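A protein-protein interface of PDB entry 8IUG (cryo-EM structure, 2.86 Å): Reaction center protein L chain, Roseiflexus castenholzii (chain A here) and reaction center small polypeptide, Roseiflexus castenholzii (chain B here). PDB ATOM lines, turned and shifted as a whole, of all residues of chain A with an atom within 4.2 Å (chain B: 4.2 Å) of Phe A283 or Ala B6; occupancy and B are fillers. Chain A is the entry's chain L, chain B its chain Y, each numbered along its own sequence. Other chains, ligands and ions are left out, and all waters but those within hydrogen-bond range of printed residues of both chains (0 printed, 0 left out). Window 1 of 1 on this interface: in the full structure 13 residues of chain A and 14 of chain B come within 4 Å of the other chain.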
ATOM      1  N   ALA A 177      13.776   6.332 -18.227  1.00  0.00           N
ATOM      2  CA  ALA A 177      13.079   5.495 -17.254  1.00  0.00           C
ATOM      3  C   ALA A 177      13.151   4.020 -17.628  1.00  0.00           C
ATOM      4  O   ALA A 177      13.354   3.165 -16.759  1.00  0.00           O
ATOM      5  CB  ALA A 177      11.628   5.944 -17.120  1.00  0.00           C
ATOM      6  N   ASN A 279       0.598  12.362 -23.493  1.00  0.00           N
ATOM      7  CA  ASN A 279       1.914  12.084 -22.911  1.00  0.00           C
ATOM      8  C   ASN A 279       1.853  10.911 -21.934  1.00  0.00           C
ATOM      9  O   ASN A 279       2.725  10.029 -21.944  1.00  0.00           O
ATOM     10  CB  ASN A 279       2.454  13.317 -22.196  1.00  0.00           C
ATOM     11  CG  ASN A 279       2.848  14.411 -23.140  1.00  0.00           C
ATOM     12  OD1 ASN A 279       2.701  14.281 -24.347  1.00  0.00           O
ATOM     13  ND2 ASN A 279       3.338  15.511 -22.594  1.00  0.00           N
ATOM     14  N   LEU A 280       0.825  10.889 -21.082  1.00  0.00           N
ATOM     15  CA  LEU A 280       0.737   9.901 -20.010  1.00  0.00           C
ATOM     16  C   LEU A 280       0.590   8.487 -20.549  1.00  0.00           C
ATOM     17  O   LEU A 280       1.156   7.544 -19.988  1.00  0.00           O
ATOM     18  CB  LEU A 280      -0.436  10.234 -19.088  1.00  0.00           C
ATOM     19  CG  LEU A 280      -0.203  11.234 -17.962  1.00  0.00           C
ATOM     20  CD1 LEU A 280      -1.519  11.609 -17.326  1.00  0.00           C
ATOM     21  CD2 LEU A 280       0.732  10.644 -16.930  1.00  0.00           C
ATOM     22  N   CYS A 281      -0.186   8.313 -21.618  1.00  0.00           N
ATOM     23  CA  CYS A 281      -0.414   6.974 -22.152  1.00  0.00           C
ATOM     24  C   CYS A 281       0.889   6.344 -22.630  1.00  0.00           C
ATOM     25  O   CYS A 281       1.212   5.201 -22.278  1.00  0.00           O
ATOM     26  CB  CYS A 281      -1.445   7.034 -23.280  1.00  0.00           C
ATOM     27  SG  CYS A 281      -0.890   7.719 -24.848  1.00  0.00           S
ATOM     28  N   ILE A 282       1.665   7.087 -23.417  1.00  0.00           N
ATOM     29  CA  ILE A 282       2.904   6.534 -23.941  1.00  0.00           C
ATOM     30  C   ILE A 282       3.945   6.387 -22.839  1.00  0.00           C
ATOM     31  O   ILE A 282       4.779   5.478 -22.895  1.00  0.00           O
ATOM     32  CB  ILE A 282       3.420   7.380 -25.120  1.00  0.00           C
ATOM     33  CG1 ILE A 282       4.564   6.662 -25.838  1.00  0.00           C
ATOM     34  CG2 ILE A 282       3.878   8.749 -24.654  1.00  0.00           C
ATOM     35  CD1 ILE A 282       4.233   5.275 -26.297  1.00  0.00           C
ATOM     36  N   PHE A 283       3.934   7.255 -21.823  1.00  0.00           N
ATOM     37  CA  PHE A 283       4.892   7.059 -20.739  1.00  0.00           C
ATOM     38  C   PHE A 283       4.566   5.809 -19.932  1.00  0.00           C
ATOM     39  O   PHE A 283       5.457   5.019 -19.608  1.00  0.00           O
ATOM     40  CB  PHE A 283       4.954   8.280 -19.824  1.00  0.00           C
ATOM     41  CG  PHE A 283       5.950   8.130 -18.707  1.00  0.00           C
ATOM     42  CD1 PHE A 283       7.299   8.317 -18.937  1.00  0.00           C
ATOM     43  CD2 PHE A 283       5.540   7.774 -17.438  1.00  0.00           C
ATOM     44  CE1 PHE A 283       8.210   8.164 -17.926  1.00  0.00           C
ATOM     45  CE2 PHE A 283       6.453   7.617 -16.427  1.00  0.00           C
ATOM     46  CZ  PHE A 283       7.788   7.815 -16.673  1.00  0.00           C
ATOM     47  N   LEU A 284       3.294   5.612 -19.591  1.00  0.00           N
ATOM     48  CA  LEU A 284       2.897   4.476 -18.771  1.00  0.00           C
ATOM     49  C   LEU A 284       2.832   3.168 -19.543  1.00  0.00           C
ATOM     50  O   LEU A 284       2.672   2.118 -18.920  1.00  0.00           O
ATOM     51  CB  LEU A 284       1.532   4.738 -18.128  1.00  0.00           C
ATOM     52  CG  LEU A 284       1.365   5.852 -17.096  1.00  0.00           C
ATOM     53  CD1 LEU A 284      -0.104   6.072 -16.822  1.00  0.00           C
ATOM     54  CD2 LEU A 284       2.094   5.522 -15.814  1.00  0.00           C
ATOM     55  N   SER A 285       2.909   3.198 -20.875  1.00  0.00           N
ATOM     56  CA  SER A 285       2.897   1.948 -21.630  1.00  0.00           C
ATOM     57  C   SER A 285       4.078   1.064 -21.261  1.00  0.00           C
ATOM     58  O   SER A 285       3.901  -0.105 -20.909  1.00  0.00           O
ATOM     59  CB  SER A 285       2.893   2.237 -23.124  1.00  0.00           C
ATOM     60  OG  SER A 285       1.676   2.847 -23.501  1.00  0.00           O
ATOM     61  N   GLY A 286       5.303   1.552 -21.244  1.00  0.00           N
ATOM     62  CA  GLY A 286       6.376   0.589 -20.939  1.00  0.00           C
ATOM     63  C   GLY A 286       6.861   0.500 -19.514  1.00  0.00           C
ATOM     64  O   GLY A 286       7.583  -0.443 -19.239  1.00  0.00           O
ATOM     65  N   THR A 287       6.463   1.398 -18.619  1.00  0.00           N
ATOM     66  CA  THR A 287       7.027   1.499 -17.244  1.00  0.00           C
ATOM     67  C   THR A 287       6.156   0.817 -16.185  1.00  0.00           C
ATOM     68  O   THR A 287       6.673  -0.085 -15.524  1.00  0.00           O
ATOM     69  CB  THR A 287       7.298   2.981 -16.939  1.00  0.00           C
ATOM     70  OG1 THR A 287       6.069   3.701 -17.019  1.00  0.00           O
ATOM     71  CG2 THR A 287       8.290   3.612 -17.891  1.00  0.00           C
ATOM     72  N   ILE B   4      12.526   4.527  -8.797  1.00  0.00           N
ATOM     73  CA  ILE B   4      12.853   5.861  -8.310  1.00  0.00           C
ATOM     74  C   ILE B   4      13.034   6.830  -9.465  1.00  0.00           C
ATOM     75  O   ILE B   4      12.488   7.931  -9.452  1.00  0.00           O
ATOM     76  CB  ILE B   4      14.109   5.826  -7.411  1.00  0.00           C
ATOM     77  CG1 ILE B   4      13.918   4.868  -6.244  1.00  0.00           C
ATOM     78  CG2 ILE B   4      14.415   7.208  -6.876  1.00  0.00           C
ATOM     79  CD1 ILE B   4      15.012   4.965  -5.208  1.00  0.00           C
ATOM     80  N   VAL B   5      13.799   6.425 -10.478  1.00  0.00           N
ATOM     81  CA  VAL B   5      13.916   7.219 -11.695  1.00  0.00           C
ATOM     82  C   VAL B   5      12.575   7.292 -12.411  1.00  0.00           C
ATOM     83  O   VAL B   5      12.177   8.352 -12.909  1.00  0.00           O
ATOM     84  CB  VAL B   5      15.015   6.636 -12.602  1.00  0.00           C
ATOM     85  CG1 VAL B   5      15.087   7.399 -13.912  1.00  0.00           C
ATOM     86  CG2 VAL B   5      16.347   6.673 -11.893  1.00  0.00           C
ATOM     87  N   ALA B   6      11.854   6.170 -12.464  1.00  0.00           N
ATOM     88  CA  ALA B   6      10.568   6.141 -13.152  1.00  0.00           C
ATOM     89  C   ALA B   6       9.580   7.113 -12.524  1.00  0.00           C
ATOM     90  O   ALA B   6       8.834   7.797 -13.232  1.00  0.00           O
ATOM     91  CB  ALA B   6      10.006   4.722 -13.145  1.00  0.00           C
ATOM     92  N   THR B   7       9.572   7.206 -11.192  1.00  0.00           N
ATOM     93  CA  THR B   7       8.652   8.119 -10.523  1.00  0.00           C
ATOM     94  C   THR B   7       9.074   9.576 -10.690  1.00  0.00           C
ATOM     95  O   THR B   7       8.213  10.455 -10.780  1.00  0.00           O
ATOM     96  CB  THR B   7       8.531   7.747  -9.048  1.00  0.00           C
ATOM     97  OG1 THR B   7       8.287   6.342  -8.937  1.00  0.00           O
ATOM     98  CG2 THR B   7       7.376   8.485  -8.409  1.00  0.00           C
ATOM     99  N   PHE B   8      10.377   9.857 -10.758  1.00  0.00           N
ATOM    100  CA  PHE B   8      10.823  11.213 -11.079  1.00  0.00           C
ATOM    101  C   PHE B   8      10.383  11.625 -12.480  1.00  0.00           C
ATOM    102  O   PHE B   8       9.920  12.754 -12.690  1.00  0.00           O
ATOM    103  CB  PHE B   8      12.344  11.317 -10.955  1.00  0.00           C
ATOM    104  CG  PHE B   8      12.828  11.626  -9.566  1.00  0.00           C
ATOM    105  CD1 PHE B   8      12.468  12.805  -8.939  1.00  0.00           C
ATOM    106  CD2 PHE B   8      13.662  10.749  -8.896  1.00  0.00           C
ATOM    107  CE1 PHE B   8      12.917  13.092  -7.666  1.00  0.00           C
ATOM    108  CE2 PHE B   8      14.114  11.033  -7.624  1.00  0.00           C
ATOM    109  CZ  PHE B   8      13.743  12.205  -7.010  1.00  0.00           C
ATOM    110  N   MET B   9      10.524  10.724 -13.455  1.00  0.00           N
ATOM    111  CA  MET B   9      10.094  11.037 -14.814  1.00  0.00           C
ATOM    112  C   MET B   9       8.578  11.191 -14.891  1.00  0.00           C
ATOM    113  O   MET B   9       8.069  12.036 -15.636  1.00  0.00           O
ATOM    114  CB  MET B   9      10.579   9.958 -15.779  1.00  0.00           C
ATOM    115  CG  MET B   9      12.069   9.653 -15.704  1.00  0.00           C
ATOM    116  SD  MET B   9      13.146  10.825 -16.543  1.00  0.00           S
ATOM    117  CE  MET B   9      13.777  11.766 -15.164  1.00  0.00           C
ATOM    118  N   LEU B  10       7.841  10.383 -14.128  1.00  0.00           N
ATOM    119  CA  LEU B  10       6.396  10.560 -14.041  1.00  0.00           C
ATOM    120  C   LEU B  10       6.043  11.911 -13.438  1.00  0.00           C
ATOM    121  O   LEU B  10       5.080  12.559 -13.860  1.00  0.00           O
ATOM    122  CB  LEU B  10       5.785   9.427 -13.218  1.00  0.00           C
ATOM    123  CG  LEU B  10       4.271   9.421 -13.021  1.00  0.00           C
ATOM    124  CD1 LEU B  10       3.555   9.301 -14.350  1.00  0.00           C
ATOM    125  CD2 LEU B  10       3.873   8.294 -12.093  1.00  0.00           C
ATOM    126  N   VAL B  13       6.382  14.416 -16.163  1.00  0.00           N
ATOM    127  CA  VAL B  13       5.240  14.346 -17.071  1.00  0.00           C
ATOM    128  C   VAL B  13       4.024  15.027 -16.453  1.00  0.00           C
ATOM    129  O   VAL B  13       3.239  15.680 -17.149  1.00  0.00           O
ATOM    130  CB  VAL B  13       4.946  12.881 -17.452  1.00  0.00           C
ATOM    131  CG1 VAL B  13       3.761  12.797 -18.385  1.00  0.00           C
ATOM    132  CG2 VAL B  13       6.149  12.257 -18.108  1.00  0.00           C
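Printed residues of chain B within 4 Å of Ala A177: Met B9.
Printed residues of chain B within 4 Å of Leu A280: Val B13 (3.99 Å).
Of chain B, only Ala B6, Met B9 and Leu B10 come within 4 Å of Phe A283.
Ala B6 touches just one residue of chain A: Phe A283 (3.6 Å).
Printed residues of chain A within 4 Å of Val B13: Leu A280 (3.99 Å).
The nearest residue of chain A that does not touch Ala B6 is Ala A177 (4.1 Å).
O of Phe A283 sits at hydrogen-bond distance from OG1 of Thr A287, at 3.0 Å.
Among the printed residues, merely in contact across the chains: Phe A283 with Ala B6 (3.6 Å), Phe A283 with Leu B10 (3.6 Å), Phe A283 with Met B9 (3.6 Å), Leu A280 with Val B13 (3.99 Å) and Ala A177 with Met B9 (3.99 Å).
Of the 8 printed residues of chain B, 4 touch a printed residue of chain A.
Printed residues of chain B that touch a printed residue of chain A: Ala B6, Met B9, Leu B10 and Val B13.
Among the printed residues, 5 pairs touch across the chains.
Among the printed residues, no Asp or Glu carboxylate lies within 4 Å of a Lys or Arg side-chain nitrogen of the other chain.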
